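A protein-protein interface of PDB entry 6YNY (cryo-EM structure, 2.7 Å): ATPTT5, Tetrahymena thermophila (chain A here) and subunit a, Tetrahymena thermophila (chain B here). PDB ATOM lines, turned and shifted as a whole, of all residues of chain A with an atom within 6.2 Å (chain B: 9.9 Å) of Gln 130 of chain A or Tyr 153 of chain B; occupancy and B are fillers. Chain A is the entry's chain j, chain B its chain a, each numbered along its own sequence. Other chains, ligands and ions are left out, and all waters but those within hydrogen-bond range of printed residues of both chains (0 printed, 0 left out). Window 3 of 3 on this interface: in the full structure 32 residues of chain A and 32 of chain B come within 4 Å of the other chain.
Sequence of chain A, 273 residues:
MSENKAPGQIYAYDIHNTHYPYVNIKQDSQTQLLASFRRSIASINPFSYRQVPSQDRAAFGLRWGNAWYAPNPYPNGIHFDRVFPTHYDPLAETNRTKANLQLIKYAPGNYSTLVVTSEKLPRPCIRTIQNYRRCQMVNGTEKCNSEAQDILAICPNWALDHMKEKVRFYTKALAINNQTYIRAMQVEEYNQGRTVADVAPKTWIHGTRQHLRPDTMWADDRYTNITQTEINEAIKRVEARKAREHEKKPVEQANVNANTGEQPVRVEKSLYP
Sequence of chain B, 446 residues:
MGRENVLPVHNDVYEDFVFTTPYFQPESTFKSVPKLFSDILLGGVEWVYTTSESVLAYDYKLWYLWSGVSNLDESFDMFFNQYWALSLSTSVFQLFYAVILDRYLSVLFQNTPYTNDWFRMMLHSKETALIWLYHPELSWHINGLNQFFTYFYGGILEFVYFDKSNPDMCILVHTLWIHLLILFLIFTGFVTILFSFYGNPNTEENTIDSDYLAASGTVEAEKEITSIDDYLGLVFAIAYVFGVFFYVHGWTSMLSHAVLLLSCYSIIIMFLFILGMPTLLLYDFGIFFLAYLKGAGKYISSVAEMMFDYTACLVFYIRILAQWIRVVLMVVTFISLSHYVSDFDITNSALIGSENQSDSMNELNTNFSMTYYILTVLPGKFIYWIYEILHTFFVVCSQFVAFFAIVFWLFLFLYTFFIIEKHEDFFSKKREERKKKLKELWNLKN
The backbone carbonyl oxygen (O) of Thr 150 of chain B lies within hydrogen-bond range of the side-chain amino group (NZ) of Lys 166 of chain A, at 2.9 Å.
The backbone carbonyl oxygen (O) of Tyr 151 of chain B lies within hydrogen-bond range of the side-chain amino group (NZ) of Lys 166 of chain A.
OH of Tyr 153 of chain B is in hydrogen-bond range of NH2 of Arg 133 of chain A.
The side-chain amino group of Lys 166 of chain A lies within hydrogen-bond range of the backbone carbonyl oxygen of Gly 154 of chain B (2.5 Å).
The backbone NH (N) of Gly 155 of chain B lies within hydrogen-bond range of the backbone carbonyl oxygen (O) of Glu 119 of chain A, at 2.7 Å.
Of the 15 printed residues of chain A, 7 touch a printed residue of chain B.
Hydrophobic or aromatic side chains of chain A that line the printed part of chain B: Leu 121, Ile 126 and Ile 129.
Hydrophobic or aromatic side chains of chain B within 4 Å of the printed part of chain A: Phe 148, Phe 152 and Tyr 153.
Among the printed residues, 14 pairs touch across the chains.
Among the printed residues, no Asp or Glu carboxylate lies within 4 Å of a Lys or Arg side-chain nitrogen of the other chain.
The side-chain hydroxyl (OH) of Tyr 114 of chain B is in hydrogen-bond range of the backbone carbonyl oxygen (O) of Tyr 153 of chain B (3.5 Å).
N of Gly 154 of chain B sits at hydrogen-bond distance from O of Phe 149 of chain B.
Among the printed residues, pairs that only touch across the chains: Glu 119 of chain A with Gly 154 of chain B (3.6 Å), Leu 121 of chain A with Tyr 153 of chain B (3.7 Å), Leu 121 of chain A with Gly 154 of chain B (3.4 Å), Ile 126 of chain A with Tyr 153 of chain B (3.6 Å), Ile 129 of chain A with Phe 152 of chain B (3.3 Å), Gln 130 of chain A with Tyr 153 of chain B (3.4 Å), Arg 133 of chain A with Phe 148 of chain B (3.9 Å), Arg 133 of chain A with Phe 152 of chain B (3.7 Å) and Lys 166 of chain A with Gly 155 of chain B (3.6 Å).
Gln 130 of chain A touches one residue of chain B.
Tyr 153 of chain B touches just these residues of chain A: Leu 121 (3.7 Å), Ile 126 (3.6 Å), Gln 130 (3.4 Å) and Arg 133 (3.0 Å).
Of chain B, only Tyr 153 (3.7 Å) and Gly 154 (3.4 Å) come within 4 Å of Leu 121 of chain A.
Ile 126 of chain A touches one residue of chain B.
No residue of chain B comes within 4 Å of Arg 127 of chain A.
Ile 129 of chain A touches one residue of chain B.
Of chain B, only Phe 148, Phe 152 and Tyr 153 come within 4 Å of Arg 133 of chain A.
Printed residues of chain A within 4 Å of Gly 154 of chain B: Glu 119 (3.6 Å), Leu 121 (3.4 Å) and Lys 166 (2.5 Å).
Printed residues of chain A within 4 Å of Phe 152 of chain B: Ile 129 (3.3 Å) and Arg 133 (3.7 Å).
Of the printed residues of chain A, Tyr 151 of chain B touches Lys 166 (2.8 Å).
Lys 120 of chain A touches none of the printed residues of chain B.
The nearest residue of chain B that does not touch Gln 130 of chain A is Phe 152 of chain B (7.1 Å).
The nearest residue of chain A that does not touch Tyr 153 of chain B is Ile 129 of chain A (4.1 Å).
The nearest printed residue of chain A that does not touch Phe 152 of chain B is Lys 166 of chain A (4.2 Å).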
ATOM      1  N   GLU A 119      18.888  18.842  -5.115  1.00  0.00           N
ATOM      2  CA  GLU A 119      19.524  19.568  -4.028  1.00  0.00           C
ATOM      3  C   GLU A 119      18.978  20.987  -3.960  1.00  0.00           C
ATOM      4  O   GLU A 119      18.697  21.614  -4.984  1.00  0.00           O
ATOM      5  CB  GLU A 119      21.039  19.601  -4.225  1.00  0.00           C
ATOM      6  CG  GLU A 119      21.738  18.267  -4.019  1.00  0.00           C
ATOM      7  CD  GLU A 119      21.845  17.876  -2.555  1.00  0.00           C
ATOM      8  OE1 GLU A 119      21.127  18.468  -1.721  1.00  0.00           O
ATOM      9  OE2 GLU A 119      22.658  16.981  -2.238  1.00  0.00           O
ATOM     10  N   LYS A 120      18.827  21.490  -2.742  1.00  0.00           N
ATOM     11  CA  LYS A 120      18.304  22.829  -2.517  1.00  0.00           C
ATOM     12  C   LYS A 120      19.462  23.816  -2.451  1.00  0.00           C
ATOM     13  O   LYS A 120      20.331  23.703  -1.580  1.00  0.00           O
ATOM     14  CB  LYS A 120      17.479  22.869  -1.234  1.00  0.00           C
ATOM     15  CG  LYS A 120      16.820  24.195  -0.977  1.00  0.00           C
ATOM     16  CD  LYS A 120      15.510  24.024  -0.239  1.00  0.00           C
ATOM     17  CE  LYS A 120      15.698  23.371   1.112  1.00  0.00           C
ATOM     18  NZ  LYS A 120      14.388  23.136   1.776  1.00  0.00           N
ATOM     19  N   LEU A 121      19.476  24.776  -3.373  1.00  0.00           N
ATOM     20  CA  LEU A 121      20.576  25.717  -3.438  1.00  0.00           C
ATOM     21  C   LEU A 121      20.638  26.550  -2.160  1.00  0.00           C
ATOM     22  O   LEU A 121      19.635  26.710  -1.461  1.00  0.00           O
ATOM     23  CB  LEU A 121      20.432  26.629  -4.650  1.00  0.00           C
ATOM     24  CG  LEU A 121      20.443  25.949  -6.019  1.00  0.00           C
ATOM     25  CD1 LEU A 121      20.383  26.977  -7.111  1.00  0.00           C
ATOM     26  CD2 LEU A 121      21.663  25.077  -6.189  1.00  0.00           C
ATOM     27  N   CYS A 125      22.457  32.214  -2.225  1.00  0.00           N
ATOM     28  CA  CYS A 125      22.449  32.109  -3.677  1.00  0.00           C
ATOM     29  C   CYS A 125      21.048  32.301  -4.235  1.00  0.00           C
ATOM     30  O   CYS A 125      20.886  32.863  -5.323  1.00  0.00           O
ATOM     31  CB  CYS A 125      23.017  30.760  -4.109  1.00  0.00           C
ATOM     32  SG  CYS A 125      23.044  30.523  -5.888  1.00  0.00           S
ATOM     33  N   ILE A 126      20.030  31.842  -3.508  1.00  0.00           N
ATOM     34  CA  ILE A 126      18.654  32.035  -3.943  1.00  0.00           C
ATOM     35  C   ILE A 126      18.297  33.513  -3.934  1.00  0.00           C
ATOM     36  O   ILE A 126      17.608  34.008  -4.833  1.00  0.00           O
ATOM     37  CB  ILE A 126      17.703  31.218  -3.051  1.00  0.00           C
ATOM     38  CG1 ILE A 126      17.780  29.740  -3.423  1.00  0.00           C
ATOM     39  CG2 ILE A 126      16.290  31.742  -3.155  1.00  0.00           C
ATOM     40  CD1 ILE A 126      17.034  28.831  -2.487  1.00  0.00           C
ATOM     41  N   ARG A 127      18.763  34.242  -2.921  1.00  0.00           N
ATOM     42  CA  ARG A 127      18.447  35.659  -2.815  1.00  0.00           C
ATOM     43  C   ARG A 127      19.051  36.462  -3.959  1.00  0.00           C
ATOM     44  O   ARG A 127      18.451  37.443  -4.407  1.00  0.00           O
ATOM     45  CB  ARG A 127      18.932  36.193  -1.473  1.00  0.00           C
ATOM     46  CG  ARG A 127      18.256  35.553  -0.279  1.00  0.00           C
ATOM     47  CD  ARG A 127      16.833  36.045  -0.100  1.00  0.00           C
ATOM     48  NE  ARG A 127      15.986  35.050   0.546  1.00  0.00           N
ATOM     49  CZ  ARG A 127      15.866  34.900   1.860  1.00  0.00           C
ATOM     50  NH1 ARG A 127      16.537  35.680   2.691  1.00  0.00           N
ATOM     51  NH2 ARG A 127      15.070  33.962   2.345  1.00  0.00           N
ATOM     52  N   THR A 128      20.235  36.075  -4.437  1.00  0.00           N
ATOM     53  CA  THR A 128      20.822  36.763  -5.578  1.00  0.00           C
ATOM     54  C   THR A 128      20.006  36.539  -6.840  1.00  0.00           C
ATOM     55  O   THR A 128      19.939  37.420  -7.701  1.00  0.00           O
ATOM     56  CB  THR A 128      22.260  36.300  -5.801  1.00  0.00           C
ATOM     57  OG1 THR A 128      22.290  34.880  -5.979  1.00  0.00           O
ATOM     58  CG2 THR A 128      23.129  36.683  -4.634  1.00  0.00           C
ATOM     59  N   ILE A 129      19.384  35.368  -6.966  1.00  0.00           N
ATOM     60  CA  ILE A 129      18.550  35.088  -8.127  1.00  0.00           C
ATOM     61  C   ILE A 129      17.250  35.873  -8.042  1.00  0.00           C
ATOM     62  O   ILE A 129      16.739  36.367  -9.054  1.00  0.00           O
ATOM     63  CB  ILE A 129      18.300  33.575  -8.237  1.00  0.00           C
ATOM     64  CG1 ILE A 129      19.629  32.833  -8.349  1.00  0.00           C
ATOM     65  CG2 ILE A 129      17.430  33.262  -9.429  1.00  0.00           C
ATOM     66  CD1 ILE A 129      19.506  31.350  -8.263  1.00  0.00           C
ATOM     67  N   GLN A 130      16.692  35.999  -6.839  1.00  0.00           N
ATOM     68  CA  GLN A 130      15.478  36.784  -6.670  1.00  0.00           C
ATOM     69  C   GLN A 130      15.718  38.252  -6.976  1.00  0.00           C
ATOM     70  O   GLN A 130      14.827  38.934  -7.492  1.00  0.00           O
ATOM     71  CB  GLN A 130      14.951  36.619  -5.248  1.00  0.00           C
ATOM     72  CG  GLN A 130      14.493  35.223  -4.933  1.00  0.00           C
ATOM     73  CD  GLN A 130      13.994  35.075  -3.518  1.00  0.00           C
ATOM     74  OE1 GLN A 130      14.494  35.719  -2.597  1.00  0.00           O
ATOM     75  NE2 GLN A 130      12.997  34.226  -3.336  1.00  0.00           N
ATOM     76  N   ASN A 131      16.912  38.755  -6.663  1.00  0.00           N
ATOM     77  CA  ASN A 131      17.215  40.155  -6.931  1.00  0.00           C
ATOM     78  C   ASN A 131      17.426  40.394  -8.420  1.00  0.00           C
ATOM     79  O   ASN A 131      17.047  41.449  -8.943  1.00  0.00           O
ATOM     80  CB  ASN A 131      18.447  40.576  -6.138  1.00  0.00           C
ATOM     81  CG  ASN A 131      18.641  42.074  -6.117  1.00  0.00           C
ATOM     82  OD1 ASN A 131      18.213  42.783  -7.025  1.00  0.00           O
ATOM     83  ND2 ASN A 131      19.292  42.565  -5.073  1.00  0.00           N
ATOM     84  N   TYR A 132      18.022  39.428  -9.118  1.00  0.00           N
ATOM     85  CA  TYR A 132      18.244  39.583 -10.549  1.00  0.00           C
ATOM     86  C   TYR A 132      16.926  39.558 -11.311  1.00  0.00           C
ATOM     87  O   TYR A 132      16.661  40.434 -12.141  1.00  0.00           O
ATOM     88  CB  TYR A 132      19.181  38.489 -11.055  1.00  0.00           C
ATOM     89  CG  TYR A 132      19.381  38.497 -12.549  1.00  0.00           C
ATOM     90  CD1 TYR A 132      20.344  39.299 -13.135  1.00  0.00           C
ATOM     91  CD2 TYR A 132      18.606  37.703 -13.374  1.00  0.00           C
ATOM     92  CE1 TYR A 132      20.528  39.309 -14.496  1.00  0.00           C
ATOM     93  CE2 TYR A 132      18.782  37.708 -14.736  1.00  0.00           C
ATOM     94  CZ  TYR A 132      19.743  38.513 -15.293  1.00  0.00           C
ATOM     95  OH  TYR A 132      19.923  38.518 -16.656  1.00  0.00           O
ATOM     96  N   ARG A 133      16.087  38.558 -11.042  1.00  0.00           N
ATOM     97  CA  ARG A 133      14.793  38.485 -11.707  1.00  0.00           C
ATOM     98  C   ARG A 133      13.950  39.713 -11.403  1.00  0.00           C
ATOM     99  O   ARG A 133      13.282  40.255 -12.290  1.00  0.00           O
ATOM    100  CB  ARG A 133      14.054  37.224 -11.274  1.00  0.00           C
ATOM    101  CG  ARG A 133      14.679  35.929 -11.738  1.00  0.00           C
ATOM    102  CD  ARG A 133      13.870  34.764 -11.222  1.00  0.00           C
ATOM    103  NE  ARG A 133      12.502  34.799 -11.730  1.00  0.00           N
ATOM    104  CZ  ARG A 133      11.445  34.322 -11.083  1.00  0.00           C
ATOM    105  NH1 ARG A 133      10.246  34.405 -11.636  1.00  0.00           N
ATOM    106  NH2 ARG A 133      11.573  33.776  -9.881  1.00  0.00           N
ATOM    107  N   ARG A 134      13.967  40.163 -10.150  1.00  0.00           N
ATOM    108  CA  ARG A 134      13.196  41.337  -9.766  1.00  0.00           C
ATOM    109  C   ARG A 134      13.717  42.583 -10.466  1.00  0.00           C
ATOM    110  O   ARG A 134      12.937  43.375 -11.007  1.00  0.00           O
ATOM    111  CB  ARG A 134      13.247  41.505  -8.254  1.00  0.00           C
ATOM    112  CG  ARG A 134      12.324  42.560  -7.708  1.00  0.00           C
ATOM    113  CD  ARG A 134      12.452  42.636  -6.210  1.00  0.00           C
ATOM    114  NE  ARG A 134      13.801  43.012  -5.805  1.00  0.00           N
ATOM    115  CZ  ARG A 134      14.272  42.896  -4.570  1.00  0.00           C
ATOM    116  NH1 ARG A 134      15.513  43.268  -4.302  1.00  0.00           N
ATOM    117  NH2 ARG A 134      13.512  42.398  -3.605  1.00  0.00           N
ATOM    118  N   CYS A 135      15.035  42.779 -10.461  1.00  0.00           N
ATOM    119  CA  CYS A 135      15.620  43.908 -11.168  1.00  0.00           C
ATOM    120  C   CYS A 135      15.476  43.768 -12.676  1.00  0.00           C
ATOM    121  O   CYS A 135      15.655  44.751 -13.399  1.00  0.00           O
ATOM    122  CB  CYS A 135      17.095  44.049 -10.798  1.00  0.00           C
ATOM    123  SG  CYS A 135      17.861  45.599 -11.315  1.00  0.00           S
ATOM    124  N   LYS A 166      21.071  22.299 -15.390  1.00  0.00           N
ATOM    125  CA  LYS A 166      19.619  22.356 -15.496  1.00  0.00           C
ATOM    126  C   LYS A 166      19.190  22.854 -16.866  1.00  0.00           C
ATOM    127  O   LYS A 166      18.272  22.299 -17.481  1.00  0.00           O
ATOM    128  CB  LYS A 166      19.046  23.258 -14.406  1.00  0.00           C
ATOM    129  CG  LYS A 166      19.023  22.637 -13.031  1.00  0.00           C
ATOM    130  CD  LYS A 166      18.284  23.507 -12.037  1.00  0.00           C
ATOM    131  CE  LYS A 166      19.035  24.783 -11.732  1.00  0.00           C
ATOM    132  NZ  LYS A 166      18.322  25.644 -10.758  1.00  0.00           N
ATOM    133  N   THR B 112      11.066  15.946  -4.336  1.00  0.00           N
ATOM    134  CA  THR B 112      11.914  17.117  -4.193  1.00  0.00           C
ATOM    135  C   THR B 112      11.592  17.857  -2.906  1.00  0.00           C
ATOM    136  O   THR B 112      10.588  17.581  -2.244  1.00  0.00           O
ATOM    137  CB  THR B 112      11.734  18.043  -5.393  1.00  0.00           C
ATOM    138  OG1 THR B 112      10.357  18.409  -5.522  1.00  0.00           O
ATOM    139  CG2 THR B 112      12.203  17.365  -6.656  1.00  0.00           C
ATOM    140  N   PRO B 113      12.434  18.816  -2.515  1.00  0.00           N
ATOM    141  CA  PRO B 113      12.147  19.587  -1.295  1.00  0.00           C
ATOM    142  C   PRO B 113      10.822  20.315  -1.333  1.00  0.00           C
ATOM    143  O   PRO B 113      10.291  20.661  -0.272  1.00  0.00           O
ATOM    144  CB  PRO B 113      13.319  20.571  -1.220  1.00  0.00           C
ATOM    145  CG  PRO B 113      14.400  19.937  -2.007  1.00  0.00           C
ATOM    146  CD  PRO B 113      13.728  19.192  -3.105  1.00  0.00           C
ATOM    147  N   TYR B 114      10.273  20.565  -2.517  1.00  0.00           N
ATOM    148  CA  TYR B 114       8.989  21.227  -2.654  1.00  0.00           C
ATOM    149  C   TYR B 114       7.847  20.251  -2.892  1.00  0.00           C
ATOM    150  O   TYR B 114       6.688  20.673  -2.914  1.00  0.00           O
ATOM    151  CB  TYR B 114       9.054  22.242  -3.798  1.00  0.00           C
ATOM    152  CG  TYR B 114      10.291  23.101  -3.743  1.00  0.00           C
ATOM    153  CD1 TYR B 114      10.377  24.172  -2.870  1.00  0.00           C
ATOM    154  CD2 TYR B 114      11.378  22.836  -4.556  1.00  0.00           C
ATOM    155  CE1 TYR B 114      11.508  24.953  -2.810  1.00  0.00           C
ATOM    156  CE2 TYR B 114      12.511  23.610  -4.503  1.00  0.00           C
ATOM    157  CZ  TYR B 114      12.573  24.667  -3.628  1.00  0.00           C
ATOM    158  OH  TYR B 114      13.706  25.444  -3.573  1.00  0.00           O
ATOM    159  N   LEU B 145       4.826  23.387 -10.682  1.00  0.00           N
ATOM    160  CA  LEU B 145       5.361  24.010  -9.479  1.00  0.00           C
ATOM    161  C   LEU B 145       6.740  23.459  -9.147  1.00  0.00           C
ATOM    162  O   LEU B 145       7.678  24.217  -8.881  1.00  0.00           O
ATOM    163  CB  LEU B 145       4.389  23.784  -8.326  1.00  0.00           C
ATOM    164  CG  LEU B 145       4.743  24.344  -6.956  1.00  0.00           C
ATOM    165  CD1 LEU B 145       3.476  24.746  -6.265  1.00  0.00           C
ATOM    166  CD2 LEU B 145       5.492  23.330  -6.126  1.00  0.00           C
ATOM    167  N   ASN B 146       6.884  22.133  -9.159  1.00  0.00           N
ATOM    168  CA  ASN B 146       8.179  21.532  -8.873  1.00  0.00           C
ATOM    169  C   ASN B 146       9.214  21.936  -9.911  1.00  0.00           C
ATOM    170  O   ASN B 146      10.399  22.066  -9.590  1.00  0.00           O
ATOM    171  CB  ASN B 146       8.040  20.013  -8.806  1.00  0.00           C
ATOM    172  CG  ASN B 146       9.369  19.308  -8.661  1.00  0.00           C
ATOM    173  OD1 ASN B 146       9.943  19.257  -7.576  1.00  0.00           O
ATOM    174  ND2 ASN B 146       9.860  18.745  -9.758  1.00  0.00           N
ATOM    175  N   GLN B 147       8.786  22.141 -11.155  1.00  0.00           N
ATOM    176  CA  GLN B 147       9.701  22.567 -12.203  1.00  0.00           C
ATOM    177  C   GLN B 147      10.063  24.039 -12.077  1.00  0.00           C
ATOM    178  O   GLN B 147      11.175  24.433 -12.442  1.00  0.00           O
ATOM    179  CB  GLN B 147       9.081  22.287 -13.570  1.00  0.00           C
ATOM    180  CG  GLN B 147       9.904  22.754 -14.743  1.00  0.00           C
ATOM    181  CD  GLN B 147       9.404  22.200 -16.055  1.00  0.00           C
ATOM    182  OE1 GLN B 147       9.204  20.996 -16.197  1.00  0.00           O
ATOM    183  NE2 GLN B 147       9.195  23.078 -17.022  1.00  0.00           N
ATOM    184  N   PHE B 148       9.147  24.859 -11.562  1.00  0.00           N
ATOM    185  CA  PHE B 148       9.438  26.276 -11.386  1.00  0.00           C
ATOM    186  C   PHE B 148      10.509  26.483 -10.326  1.00  0.00           C
ATOM    187  O   PHE B 148      11.539  27.116 -10.583  1.00  0.00           O
ATOM    188  CB  PHE B 148       8.159  27.025 -11.015  1.00  0.00           C
ATOM    189  CG  PHE B 148       8.373  28.474 -10.698  1.00  0.00           C
ATOM    190  CD1 PHE B 148       8.348  29.427 -11.696  1.00  0.00           C
ATOM    191  CD2 PHE B 148       8.595  28.884  -9.399  1.00  0.00           C
ATOM    192  CE1 PHE B 148       8.544  30.753 -11.404  1.00  0.00           C
ATOM    193  CE2 PHE B 148       8.791  30.209  -9.105  1.00  0.00           C
ATOM    194  CZ  PHE B 148       8.765  31.144 -10.107  1.00  0.00           C
ATOM    195  N   PHE B 149      10.287  25.948  -9.126  1.00  0.00           N
ATOM    196  CA  PHE B 149      11.254  26.125  -8.053  1.00  0.00           C
ATOM    197  C   PHE B 149      12.540  25.364  -8.328  1.00  0.00           C
ATOM    198  O   PHE B 149      13.612  25.783  -7.883  1.00  0.00           O
ATOM    199  CB  PHE B 149      10.651  25.677  -6.729  1.00  0.00           C
ATOM    200  CG  PHE B 149       9.547  26.557  -6.239  1.00  0.00           C
ATOM    201  CD1 PHE B 149       8.230  26.204  -6.433  1.00  0.00           C
ATOM    202  CD2 PHE B 149       9.826  27.739  -5.584  1.00  0.00           C
ATOM    203  CE1 PHE B 149       7.214  27.011  -5.985  1.00  0.00           C
ATOM    204  CE2 PHE B 149       8.813  28.548  -5.136  1.00  0.00           C
ATOM    205  CZ  PHE B 149       7.507  28.184  -5.335  1.00  0.00           C
ATOM    206  N   THR B 150      12.454  24.249  -9.050  1.00  0.00           N
ATOM    207  CA  THR B 150      13.657  23.513  -9.413  1.00  0.00           C
ATOM    208  C   THR B 150      14.499  24.293 -10.410  1.00  0.00           C
ATOM    209  O   THR B 150      15.728  24.332 -10.297  1.00  0.00           O
ATOM    210  CB  THR B 150      13.278  22.151  -9.986  1.00  0.00           C
ATOM    211  OG1 THR B 150      12.588  21.387  -8.992  1.00  0.00           O
ATOM    212  CG2 THR B 150      14.502  21.399 -10.435  1.00  0.00           C
ATOM    213  N   TYR B 151      13.856  24.925 -11.390  1.00  0.00           N
ATOM    214  CA  TYR B 151      14.600  25.643 -12.416  1.00  0.00           C
ATOM    215  C   TYR B 151      15.285  26.877 -11.848  1.00  0.00           C
ATOM    216  O   TYR B 151      16.434  27.169 -12.196  1.00  0.00           O
ATOM    217  CB  TYR B 151      13.664  26.034 -13.558  1.00  0.00           C
ATOM    218  CG  TYR B 151      14.342  26.815 -14.652  1.00  0.00           C
ATOM    219  CD1 TYR B 151      15.018  26.171 -15.673  1.00  0.00           C
ATOM    220  CD2 TYR B 151      14.308  28.198 -14.662  1.00  0.00           C
ATOM    221  CE1 TYR B 151      15.641  26.881 -16.670  1.00  0.00           C
ATOM    222  CE2 TYR B 151      14.930  28.915 -15.655  1.00  0.00           C
ATOM    223  CZ  TYR B 151      15.596  28.251 -16.656  1.00  0.00           C
ATOM    224  OH  TYR B 151      16.218  28.961 -17.651  1.00  0.00           O
ATOM    225  N   PHE B 152      14.602  27.611 -10.975  1.00  0.00           N
ATOM    226  CA  PHE B 152      15.150  28.853 -10.448  1.00  0.00           C
ATOM    227  C   PHE B 152      15.949  28.662  -9.167  1.00  0.00           C
ATOM    228  O   PHE B 152      17.027  29.244  -9.024  1.00  0.00           O
ATOM    229  CB  PHE B 152      14.026  29.856 -10.184  1.00  0.00           C
ATOM    230  CG  PHE B 152      13.415  30.424 -11.421  1.00  0.00           C
ATOM    231  CD1 PHE B 152      14.165  31.186 -12.291  1.00  0.00           C
ATOM    232  CD2 PHE B 152      12.084  30.211 -11.707  1.00  0.00           C
ATOM    233  CE1 PHE B 152      13.603  31.709 -13.429  1.00  0.00           C
ATOM    234  CE2 PHE B 152      11.518  30.732 -12.842  1.00  0.00           C
ATOM    235  CZ  PHE B 152      12.277  31.484 -13.702  1.00  0.00           C
ATOM    236  N   TYR B 153      15.449  27.853  -8.233  1.00  0.00           N
ATOM    237  CA  TYR B 153      16.016  27.782  -6.893  1.00  0.00           C
ATOM    238  C   TYR B 153      16.442  26.374  -6.500  1.00  0.00           C
ATOM    239  O   TYR B 153      16.654  26.110  -5.314  1.00  0.00           O
ATOM    240  CB  TYR B 153      15.012  28.313  -5.871  1.00  0.00           C
ATOM    241  CG  TYR B 153      14.412  29.645  -6.231  1.00  0.00           C
ATOM    242  CD1 TYR B 153      15.212  30.757  -6.411  1.00  0.00           C
ATOM    243  CD2 TYR B 153      13.045  29.793  -6.375  1.00  0.00           C
ATOM    244  CE1 TYR B 153      14.670  31.975  -6.732  1.00  0.00           C
ATOM    245  CE2 TYR B 153      12.495  31.009  -6.697  1.00  0.00           C
ATOM    246  CZ  TYR B 153      13.310  32.098  -6.874  1.00  0.00           C
ATOM    247  OH  TYR B 153      12.763  33.317  -7.196  1.00  0.00           O
ATOM    248  N   GLY B 154      16.580  25.464  -7.461  1.00  0.00           N
ATOM    249  CA  GLY B 154      16.917  24.091  -7.176  1.00  0.00           C
ATOM    250  C   GLY B 154      18.186  23.633  -7.871  1.00  0.00           C
ATOM    251  O   GLY B 154      18.813  24.364  -8.641  1.00  0.00           O
ATOM    252  N   GLY B 155      18.552  22.388  -7.573  1.00  0.00           N
ATOM    253  CA  GLY B 155      19.696  21.748  -8.174  1.00  0.00           C
ATOM    254  C   GLY B 155      19.304  20.787  -9.281  1.00  0.00           C
ATOM    255  O   GLY B 155      18.166  20.759  -9.756  1.00  0.00           O
ATOM    256  N   ILE B 156      20.279  19.980  -9.691  1.00  0.00           N
ATOM    257  CA  ILE B 156      20.046  19.014 -10.752  1.00  0.00           C
ATOM    258  C   ILE B 156      19.073  17.947 -10.269  1.00  0.00           C
ATOM    259  O   ILE B 156      19.010  17.617  -9.078  1.00  0.00           O
ATOM    260  CB  ILE B 156      21.372  18.383 -11.212  1.00  0.00           C
ATOM    261  CG1 ILE B 156      22.356  19.465 -11.644  1.00  0.00           C
ATOM    262  CG2 ILE B 156      21.127  17.439 -12.366  1.00  0.00           C
ATOM    263  CD1 ILE B 156      23.754  18.955 -11.874  1.00  0.00           C
